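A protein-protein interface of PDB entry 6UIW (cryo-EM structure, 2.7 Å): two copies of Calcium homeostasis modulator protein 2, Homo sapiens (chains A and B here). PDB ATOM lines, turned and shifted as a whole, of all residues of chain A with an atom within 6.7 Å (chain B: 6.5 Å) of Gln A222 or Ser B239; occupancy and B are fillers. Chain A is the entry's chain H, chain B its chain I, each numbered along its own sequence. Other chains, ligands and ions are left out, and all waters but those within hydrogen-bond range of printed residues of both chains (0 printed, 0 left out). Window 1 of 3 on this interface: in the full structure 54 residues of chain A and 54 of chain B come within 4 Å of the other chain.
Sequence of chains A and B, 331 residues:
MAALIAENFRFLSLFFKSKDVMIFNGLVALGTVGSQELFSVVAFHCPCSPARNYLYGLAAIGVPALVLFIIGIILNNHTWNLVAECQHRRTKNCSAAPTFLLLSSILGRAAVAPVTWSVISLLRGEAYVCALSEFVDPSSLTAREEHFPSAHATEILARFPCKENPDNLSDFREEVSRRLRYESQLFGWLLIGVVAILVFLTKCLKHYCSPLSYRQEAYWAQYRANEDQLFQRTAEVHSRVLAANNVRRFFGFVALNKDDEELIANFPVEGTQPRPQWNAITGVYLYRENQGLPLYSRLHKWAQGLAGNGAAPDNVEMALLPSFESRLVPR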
ATOM      1  N   GLU A 217     -11.748   7.174  15.719  1.00  0.00           N
ATOM      2  CA  GLU A 217     -12.888   7.303  14.821  1.00  0.00           C
ATOM      3  C   GLU A 217     -12.584   6.683  13.470  1.00  0.00           C
ATOM      4  O   GLU A 217     -13.479   6.143  12.814  1.00  0.00           O
ATOM      5  CB  GLU A 217     -13.278   8.767  14.669  1.00  0.00           C
ATOM      6  N   ALA A 218     -11.318   6.682  13.062  1.00  0.00           N
ATOM      7  CA  ALA A 218     -10.955   5.982  11.836  1.00  0.00           C
ATOM      8  C   ALA A 218     -11.010   4.478  12.032  1.00  0.00           C
ATOM      9  O   ALA A 218     -11.413   3.736  11.128  1.00  0.00           O
ATOM     10  CB  ALA A 218      -9.567   6.410  11.377  1.00  0.00           C
ATOM     11  N   TYR A 219     -10.633   4.014  13.221  1.00  0.00           N
ATOM     12  CA  TYR A 219     -10.772   2.600  13.539  1.00  0.00           C
ATOM     13  C   TYR A 219     -12.232   2.198  13.619  1.00  0.00           C
ATOM     14  O   TYR A 219     -12.603   1.094  13.223  1.00  0.00           O
ATOM     15  CB  TYR A 219     -10.080   2.301  14.857  1.00  0.00           C
ATOM     16  CG  TYR A 219     -10.269   0.898  15.339  1.00  0.00           C
ATOM     17  CD1 TYR A 219      -9.540  -0.132  14.797  1.00  0.00           C
ATOM     18  CD2 TYR A 219     -11.156   0.607  16.352  1.00  0.00           C
ATOM     19  CE1 TYR A 219      -9.699  -1.410  15.235  1.00  0.00           C
ATOM     20  CE2 TYR A 219     -11.325  -0.671  16.791  1.00  0.00           C
ATOM     21  CZ  TYR A 219     -10.592  -1.673  16.231  1.00  0.00           C
ATOM     22  OH  TYR A 219     -10.753  -2.954  16.673  1.00  0.00           O
ATOM     23  N   TRP A 220     -13.070   3.082  14.143  1.00  0.00           N
ATOM     24  CA  TRP A 220     -14.498   2.831  14.219  1.00  0.00           C
ATOM     25  C   TRP A 220     -15.110   2.759  12.834  1.00  0.00           C
ATOM     26  O   TRP A 220     -15.982   1.930  12.582  1.00  0.00           O
ATOM     27  CB  TRP A 220     -15.143   3.937  15.036  1.00  0.00           C
ATOM     28  CG  TRP A 220     -16.514   3.693  15.462  1.00  0.00           C
ATOM     29  CD1 TRP A 220     -17.227   2.558  15.317  1.00  0.00           C
ATOM     30  CD2 TRP A 220     -17.354   4.614  16.134  1.00  0.00           C
ATOM     31  NE1 TRP A 220     -18.473   2.712  15.844  1.00  0.00           N
ATOM     32  CE2 TRP A 220     -18.574   3.974  16.359  1.00  0.00           C
ATOM     33  CE3 TRP A 220     -17.195   5.925  16.568  1.00  0.00           C
ATOM     34  CZ2 TRP A 220     -19.629   4.593  17.000  1.00  0.00           C
ATOM     35  CZ3 TRP A 220     -18.237   6.538  17.200  1.00  0.00           C
ATOM     36  CH2 TRP A 220     -19.439   5.874  17.413  1.00  0.00           C
ATOM     37  N   ALA A 221     -14.658   3.615  11.922  1.00  0.00           N
ATOM     38  CA  ALA A 221     -15.159   3.556  10.558  1.00  0.00           C
ATOM     39  C   ALA A 221     -14.717   2.277   9.870  1.00  0.00           C
ATOM     40  O   ALA A 221     -15.496   1.662   9.131  1.00  0.00           O
ATOM     41  CB  ALA A 221     -14.683   4.774   9.777  1.00  0.00           C
ATOM     42  N   GLN A 222     -13.491   1.836  10.140  1.00  0.00           N
ATOM     43  CA  GLN A 222     -13.026   0.577   9.571  1.00  0.00           C
ATOM     44  C   GLN A 222     -13.775  -0.601  10.164  1.00  0.00           C
ATOM     45  O   GLN A 222     -14.061  -1.578   9.463  1.00  0.00           O
ATOM     46  CB  GLN A 222     -11.533   0.421   9.799  1.00  0.00           C
ATOM     47  CG  GLN A 222     -10.699   1.055   8.737  1.00  0.00           C
ATOM     48  CD  GLN A 222      -9.304   1.316   9.214  1.00  0.00           C
ATOM     49  OE1 GLN A 222      -8.821   0.647  10.118  1.00  0.00           O
ATOM     50  NE2 GLN A 222      -8.639   2.286   8.609  1.00  0.00           N
ATOM     51  N   TYR A 223     -14.125  -0.514  11.445  1.00  0.00           N
ATOM     52  CA  TYR A 223     -14.912  -1.561  12.074  1.00  0.00           C
ATOM     53  C   TYR A 223     -16.297  -1.627  11.482  1.00  0.00           C
ATOM     54  O   TYR A 223     -16.828  -2.714  11.275  1.00  0.00           O
ATOM     55  CB  TYR A 223     -15.020  -1.336  13.575  1.00  0.00           C
ATOM     56  CG  TYR A 223     -15.960  -2.311  14.236  1.00  0.00           C
ATOM     57  CD1 TYR A 223     -15.551  -3.587  14.523  1.00  0.00           C
ATOM     58  CD2 TYR A 223     -17.260  -1.961  14.563  1.00  0.00           C
ATOM     59  CE1 TYR A 223     -16.391  -4.481  15.114  1.00  0.00           C
ATOM     60  CE2 TYR A 223     -18.106  -2.853  15.142  1.00  0.00           C
ATOM     61  CZ  TYR A 223     -17.666  -4.111  15.416  1.00  0.00           C
ATOM     62  OH  TYR A 223     -18.510  -5.007  16.005  1.00  0.00           O
ATOM     63  N   ARG A 224     -16.929  -0.477  11.280  1.00  0.00           N
ATOM     64  CA  ARG A 224     -18.285  -0.469  10.764  1.00  0.00           C
ATOM     65  C   ARG A 224     -18.324  -0.987   9.343  1.00  0.00           C
ATOM     66  O   ARG A 224     -19.236  -1.734   8.979  1.00  0.00           O
ATOM     67  CB  ARG A 224     -18.860   0.932  10.844  1.00  0.00           C
ATOM     68  CG  ARG A 224     -19.214   1.325  12.239  1.00  0.00           C
ATOM     69  CD  ARG A 224     -20.022   2.579  12.225  1.00  0.00           C
ATOM     70  NE  ARG A 224     -19.432   3.556  11.328  1.00  0.00           N
ATOM     71  CZ  ARG A 224     -18.705   4.586  11.736  1.00  0.00           C
ATOM     72  NH1 ARG A 224     -18.202   5.432  10.854  1.00  0.00           N
ATOM     73  NH2 ARG A 224     -18.486   4.769  13.027  1.00  0.00           N
ATOM     74  N   ALA A 225     -17.302  -0.668   8.548  1.00  0.00           N
ATOM     75  CA  ALA A 225     -17.232  -1.207   7.197  1.00  0.00           C
ATOM     76  C   ALA A 225     -17.011  -2.714   7.216  1.00  0.00           C
ATOM     77  O   ALA A 225     -17.691  -3.457   6.497  1.00  0.00           O
ATOM     78  CB  ALA A 225     -16.124  -0.511   6.417  1.00  0.00           C
ATOM     79  N   ASN A 226     -16.102  -3.187   8.074  1.00  0.00           N
ATOM     80  CA  ASN A 226     -15.838  -4.618   8.159  1.00  0.00           C
ATOM     81  C   ASN A 226     -17.030  -5.365   8.717  1.00  0.00           C
ATOM     82  O   ASN A 226     -17.322  -6.481   8.289  1.00  0.00           O
ATOM     83  CB  ASN A 226     -14.623  -4.883   9.035  1.00  0.00           C
ATOM     84  CG  ASN A 226     -13.341  -4.522   8.359  1.00  0.00           C
ATOM     85  OD1 ASN A 226     -12.333  -4.293   9.013  1.00  0.00           O
ATOM     86  ND2 ASN A 226     -13.366  -4.459   7.040  1.00  0.00           N
ATOM     87  N   GLU A 227     -17.763  -4.752   9.635  1.00  0.00           N
ATOM     88  CA  GLU A 227     -18.861  -5.450  10.269  1.00  0.00           C
ATOM     89  C   GLU A 227     -20.062  -5.513   9.356  1.00  0.00           C
ATOM     90  O   GLU A 227     -20.729  -6.544   9.287  1.00  0.00           O
ATOM     91  CB  GLU A 227     -19.217  -4.783  11.584  1.00  0.00           C
ATOM     92  CG  GLU A 227     -20.206  -5.567  12.370  1.00  0.00           C
ATOM     93  CD  GLU A 227     -21.037  -4.698  13.259  1.00  0.00           C
ATOM     94  OE1 GLU A 227     -20.732  -4.629  14.463  1.00  0.00           O
ATOM     95  OE2 GLU A 227     -21.985  -4.071  12.755  1.00  0.00           O
ATOM     96  N   LEU A 230     -18.989  -8.138   6.617  1.00  0.00           N
ATOM     97  CA  LEU A 230     -19.002  -9.495   7.136  1.00  0.00           C
ATOM     98  C   LEU A 230     -20.404  -9.928   7.496  1.00  0.00           C
ATOM     99  O   LEU A 230     -20.749 -11.097   7.325  1.00  0.00           O
ATOM    100  CB  LEU A 230     -18.101  -9.602   8.357  1.00  0.00           C
ATOM    101  CG  LEU A 230     -16.616  -9.722   8.086  1.00  0.00           C
ATOM    102  CD1 LEU A 230     -15.906  -9.891   9.389  1.00  0.00           C
ATOM    103  CD2 LEU A 230     -16.352 -10.896   7.187  1.00  0.00           C
ATOM    104  N   PHE B 231      -0.151   1.149  10.787  1.00  0.00           N
ATOM    105  CA  PHE B 231      -1.245   1.332  11.721  1.00  0.00           C
ATOM    106  C   PHE B 231      -2.587   1.255  11.022  1.00  0.00           C
ATOM    107  O   PHE B 231      -3.526   0.674  11.564  1.00  0.00           O
ATOM    108  CB  PHE B 231      -1.097   2.661  12.443  1.00  0.00           C
ATOM    109  CG  PHE B 231      -1.904   2.752  13.682  1.00  0.00           C
ATOM    110  CD1 PHE B 231      -1.383   2.339  14.882  1.00  0.00           C
ATOM    111  CD2 PHE B 231      -3.189   3.243  13.651  1.00  0.00           C
ATOM    112  CE1 PHE B 231      -2.122   2.414  16.018  1.00  0.00           C
ATOM    113  CE2 PHE B 231      -3.929   3.315  14.786  1.00  0.00           C
ATOM    114  CZ  PHE B 231      -3.396   2.897  15.966  1.00  0.00           C
ATOM    115  N   GLN B 232      -2.704   1.828   9.823  1.00  0.00           N
ATOM    116  CA  GLN B 232      -3.947   1.696   9.075  1.00  0.00           C
ATOM    117  C   GLN B 232      -4.199   0.253   8.681  1.00  0.00           C
ATOM    118  O   GLN B 232      -5.334  -0.228   8.768  1.00  0.00           O
ATOM    119  CB  GLN B 232      -3.931   2.578   7.833  1.00  0.00           C
ATOM    120  CG  GLN B 232      -3.996   4.061   8.098  1.00  0.00           C
ATOM    121  CD  GLN B 232      -4.908   4.420   9.246  1.00  0.00           C
ATOM    122  OE1 GLN B 232      -4.452   4.903  10.279  1.00  0.00           O
ATOM    123  NE2 GLN B 232      -6.207   4.212   9.063  1.00  0.00           N
ATOM    124  N   ARG B 233      -3.143  -0.468   8.290  1.00  0.00           N
ATOM    125  CA  ARG B 233      -3.322  -1.863   7.898  1.00  0.00           C
ATOM    126  C   ARG B 233      -3.738  -2.724   9.076  1.00  0.00           C
ATOM    127  O   ARG B 233      -4.689  -3.505   8.979  1.00  0.00           O
ATOM    128  CB  ARG B 233      -2.048  -2.416   7.284  1.00  0.00           C
ATOM    129  CG  ARG B 233      -1.849  -2.055   5.842  1.00  0.00           C
ATOM    130  CD  ARG B 233      -0.573  -2.688   5.342  1.00  0.00           C
ATOM    131  NE  ARG B 233      -0.227  -2.271   3.989  1.00  0.00           N
ATOM    132  CZ  ARG B 233       0.937  -2.543   3.415  1.00  0.00           C
ATOM    133  NH1 ARG B 233       1.855  -3.230   4.081  1.00  0.00           N
ATOM    134  NH2 ARG B 233       1.184  -2.134   2.178  1.00  0.00           N
ATOM    135  N   THR B 234      -3.076  -2.573  10.216  1.00  0.00           N
ATOM    136  CA  THR B 234      -3.442  -3.443  11.319  1.00  0.00           C
ATOM    137  C   THR B 234      -4.687  -2.945  12.032  1.00  0.00           C
ATOM    138  O   THR B 234      -5.331  -3.711  12.740  1.00  0.00           O
ATOM    139  CB  THR B 234      -2.296  -3.596  12.294  1.00  0.00           C
ATOM    140  OG1 THR B 234      -2.654  -4.569  13.274  1.00  0.00           O
ATOM    141  CG2 THR B 234      -2.108  -2.358  12.980  1.00  0.00           C
ATOM    142  N   ALA B 235      -5.089  -1.695  11.809  1.00  0.00           N
ATOM    143  CA  ALA B 235      -6.363  -1.260  12.346  1.00  0.00           C
ATOM    144  C   ALA B 235      -7.494  -1.844  11.532  1.00  0.00           C
ATOM    145  O   ALA B 235      -8.503  -2.277  12.093  1.00  0.00           O
ATOM    146  CB  ALA B 235      -6.435   0.260  12.370  1.00  0.00           C
ATOM    147  N   GLU B 236      -7.323  -1.907  10.207  1.00  0.00           N
ATOM    148  CA  GLU B 236      -8.296  -2.590   9.365  1.00  0.00           C
ATOM    149  C   GLU B 236      -8.381  -4.067   9.705  1.00  0.00           C
ATOM    150  O   GLU B 236      -9.477  -4.622   9.817  1.00  0.00           O
ATOM    151  CB  GLU B 236      -7.941  -2.402   7.894  1.00  0.00           C
ATOM    152  N   VAL B 237      -7.238  -4.705   9.950  1.00  0.00           N
ATOM    153  CA  VAL B 237      -7.242  -6.136  10.237  1.00  0.00           C
ATOM    154  C   VAL B 237      -7.814  -6.412  11.623  1.00  0.00           C
ATOM    155  O   VAL B 237      -8.624  -7.325  11.800  1.00  0.00           O
ATOM    156  CB  VAL B 237      -5.824  -6.701  10.061  1.00  0.00           C
ATOM    157  CG1 VAL B 237      -5.638  -7.989  10.807  1.00  0.00           C
ATOM    158  CG2 VAL B 237      -5.566  -6.920   8.599  1.00  0.00           C
ATOM    159  N   HIS B 238      -7.448  -5.599  12.609  1.00  0.00           N
ATOM    160  CA  HIS B 238      -7.948  -5.762  13.965  1.00  0.00           C
ATOM    161  C   HIS B 238      -9.441  -5.500  14.037  1.00  0.00           C
ATOM    162  O   HIS B 238     -10.172  -6.207  14.740  1.00  0.00           O
ATOM    163  CB  HIS B 238      -7.189  -4.800  14.861  1.00  0.00           C
ATOM    164  CG  HIS B 238      -7.486  -4.925  16.316  1.00  0.00           C
ATOM    165  ND1 HIS B 238      -8.655  -4.471  16.879  1.00  0.00           N
ATOM    166  CD2 HIS B 238      -6.726  -5.368  17.338  1.00  0.00           C
ATOM    167  CE1 HIS B 238      -8.619  -4.669  18.181  1.00  0.00           C
ATOM    168  NE2 HIS B 238      -7.447  -5.184  18.489  1.00  0.00           N
ATOM    169  N   SER B 239      -9.918  -4.520  13.277  1.00  0.00           N
ATOM    170  CA  SER B 239     -11.344  -4.255  13.228  1.00  0.00           C
ATOM    171  C   SER B 239     -12.078  -5.369  12.515  1.00  0.00           C
ATOM    172  O   SER B 239     -13.206  -5.700  12.876  1.00  0.00           O
ATOM    173  CB  SER B 239     -11.587  -2.934  12.524  1.00  0.00           C
ATOM    174  OG  SER B 239     -11.191  -3.031  11.177  1.00  0.00           O
ATOM    175  N   ARG B 240     -11.442  -5.979  11.515  1.00  0.00           N
ATOM    176  CA  ARG B 240     -12.067  -7.096  10.821  1.00  0.00           C
ATOM    177  C   ARG B 240     -12.186  -8.316  11.718  1.00  0.00           C
ATOM    178  O   ARG B 240     -13.199  -9.018  11.682  1.00  0.00           O
ATOM    179  CB  ARG B 240     -11.278  -7.439   9.570  1.00  0.00           C
ATOM    180  CG  ARG B 240     -11.992  -8.375   8.657  1.00  0.00           C
ATOM    181  CD  ARG B 240     -11.633  -8.085   7.232  1.00  0.00           C
ATOM    182  NE  ARG B 240     -12.414  -8.903   6.316  1.00  0.00           N
ATOM    183  CZ  ARG B 240     -13.527  -8.494   5.724  1.00  0.00           C
ATOM    184  NH1 ARG B 240     -13.993  -7.277   5.951  1.00  0.00           N
ATOM    185  NH2 ARG B 240     -14.178  -9.301   4.903  1.00  0.00           N
ATOM    186  N   VAL B 241     -11.185  -8.575  12.553  1.00  0.00           N
ATOM    187  CA  VAL B 241     -11.272  -9.746  13.419  1.00  0.00           C
ATOM    188  C   VAL B 241     -12.246  -9.487  14.561  1.00  0.00           C
ATOM    189  O   VAL B 241     -12.963 -10.393  14.998  1.00  0.00           O
ATOM    190  CB  VAL B 241      -9.880 -10.157  13.925  1.00  0.00           C
ATOM    191  CG1 VAL B 241      -9.955 -11.456  14.669  1.00  0.00           C
ATOM    192  CG2 VAL B 241      -8.962 -10.361  12.772  1.00  0.00           C
ATOM    193  N   LEU B 242     -12.345  -8.236  15.013  1.00  0.00           N
ATOM    194  CA  LEU B 242     -13.346  -7.912  16.024  1.00  0.00           C
ATOM    195  C   LEU B 242     -14.755  -8.013  15.457  1.00  0.00           C
ATOM    196  O   LEU B 242     -15.676  -8.509  16.123  1.00  0.00           O
ATOM    197  CB  LEU B 242     -13.093  -6.515  16.567  1.00  0.00           C
ATOM    198  CG  LEU B 242     -14.001  -6.126  17.717  1.00  0.00           C
ATOM    199  CD1 LEU B 242     -13.700  -6.992  18.911  1.00  0.00           C
ATOM    200  CD2 LEU B 242     -13.805  -4.676  18.043  1.00  0.00           C
ATOM    201  N   ALA B 243     -14.929  -7.574  14.213  1.00  0.00           N
ATOM    202  CA  ALA B 243     -16.210  -7.695  13.540  1.00  0.00           C
ATOM    203  C   ALA B 243     -16.575  -9.146  13.318  1.00  0.00           C
ATOM    204  O   ALA B 243     -17.742  -9.520  13.441  1.00  0.00           O
ATOM    205  CB  ALA B 243     -16.158  -6.951  12.215  1.00  0.00           C
ATOM    206  N   ALA B 244     -15.588  -9.982  13.007  1.00  0.00           N
ATOM    207  CA  ALA B 244     -15.857 -11.399  12.841  1.00  0.00           C
ATOM    208  C   ALA B 244     -16.223 -12.050  14.162  1.00  0.00           C
ATOM    209  O   ALA B 244     -17.065 -12.944  14.194  1.00  0.00           O
ATOM    210  CB  ALA B 244     -14.652 -12.088  12.220  1.00  0.00           C
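The side-chain amide oxygen of Asn A226 lies within hydrogen-bond range of the side-chain hydroxyl of Ser B239 (2.8 Å).
The backbone NH (N) of Glu B236 sits at hydrogen-bond distance from the side-chain amide oxygen (OE1) of Gln A222, 3.0 Å away.
The side-chain amide nitrogen (NE2) of Gln A222 lies close to the side-chain amide nitrogen (NE2) of Gln B232 (3.1 Å).
The side-chain amide oxygen (OD1) of Asn A226 lies close to the backbone carbonyl oxygen (O) of Glu B236 (3.0 Å).
ND2 of Asn A226 lies close to NH1 of Arg B240, 3.1 Å away.
ND1 of His B238 lies within hydrogen-bond range of OH of Tyr A219 (2.6 Å).
The side-chain hydroxyl of Tyr A223 lies within hydrogen-bond range of the side-chain carboxylate of Glu A227 (2.7 Å).
O of Glu B236 lies within hydrogen-bond range of OG of Ser B239.
The side-chain hydroxyl (OG) of Ser B239 sits at hydrogen-bond distance from the backbone carbonyl oxygen (O) of Ala B235 (2.9 Å).
OD1 of Asn A226 lies close to O of Gln A222 (3.2 Å).
Gln A222 touches just these residues of chain B: Gln B232, Ala B235, Glu B236 and Ser B239.
Ser B239 touches just these residues of chain A: Tyr A219, Gln A222, Tyr A223 and Asn A226.
Of the printed residues of chain B, Tyr A223 touches Ser B239, Leu B242 and Ala B243.
Printed residues of chain A within 4 Å of Gln B232: Gln A222.
Of the printed residues of chain B, Glu A227 touches Ala B243 (3.7 Å).
Of the printed residues of chain A, Arg B240 touches Asn A226 and Leu A230.
Printed residues of chain B within 4 Å of Asn A226: Glu B236, Ser B239, Arg B240 and Ala B243.
The nearest printed residue of chain B that does not touch Gln A222 is Phe B231 (5.5 Å).
The nearest residue of chain A that does not touch Ser B239 is Glu A227 (5.7 Å).
The nearest printed residue of chain A that does not touch Ala B244 is Tyr A223 (5.9 Å).
No position is printed for both chains.
Of the 18 pairs that touch across the chains among the printed residues, none has its exchanged pair printed and touching as well.
Of the 14 printed residues of chain B, 9 touch a printed residue of chain A.
Hydrophobic or aromatic side chains of chain B within 4 Å of the printed part of chain A: Ala B235, His B238, Leu B242, Ala B243 and Ala B244.
Printed residues of chain A that touch a printed residue of chain B: Tyr A219, Gln A222, Tyr A223, Asn A226, Glu A227 and Leu A230.
Hydrophobic or aromatic side chains of chain A that line the printed part of chain B: Tyr A219, Tyr A223 and Leu A230.
Among the printed residues, 18 pairs touch across the chains.
Among the printed residues, no Asp or Glu carboxylate lies within 4 Å of a Lys or Arg side-chain nitrogen of the other chain.
CE1 of Tyr A219 touches O of Ala B235, at 3.5 Å.
CE1 of Tyr A219 touches CB of Ser B239, at 3.6 Å.
Tyr A219 touches Leu B242 (OH to CD2, 3.8 Å).
Gln A222 touches Ala B235 (OE1 to C, 3.2 Å).
OG of Ser B239 touches O of Gln A222, 3.6 Å away.
Ser B239 touches Tyr A223.
Tyr A223 touches Ala B243 (CE1 to N, 3.5 Å).
C of Asn A226 touches CB of Ala B243, 3.9 Å away.
CA of Glu A227 touches CB of Ala B243, at 3.7 Å.
NH2 of Arg B240 touches CD2 of Leu A230, at 3.5 Å.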
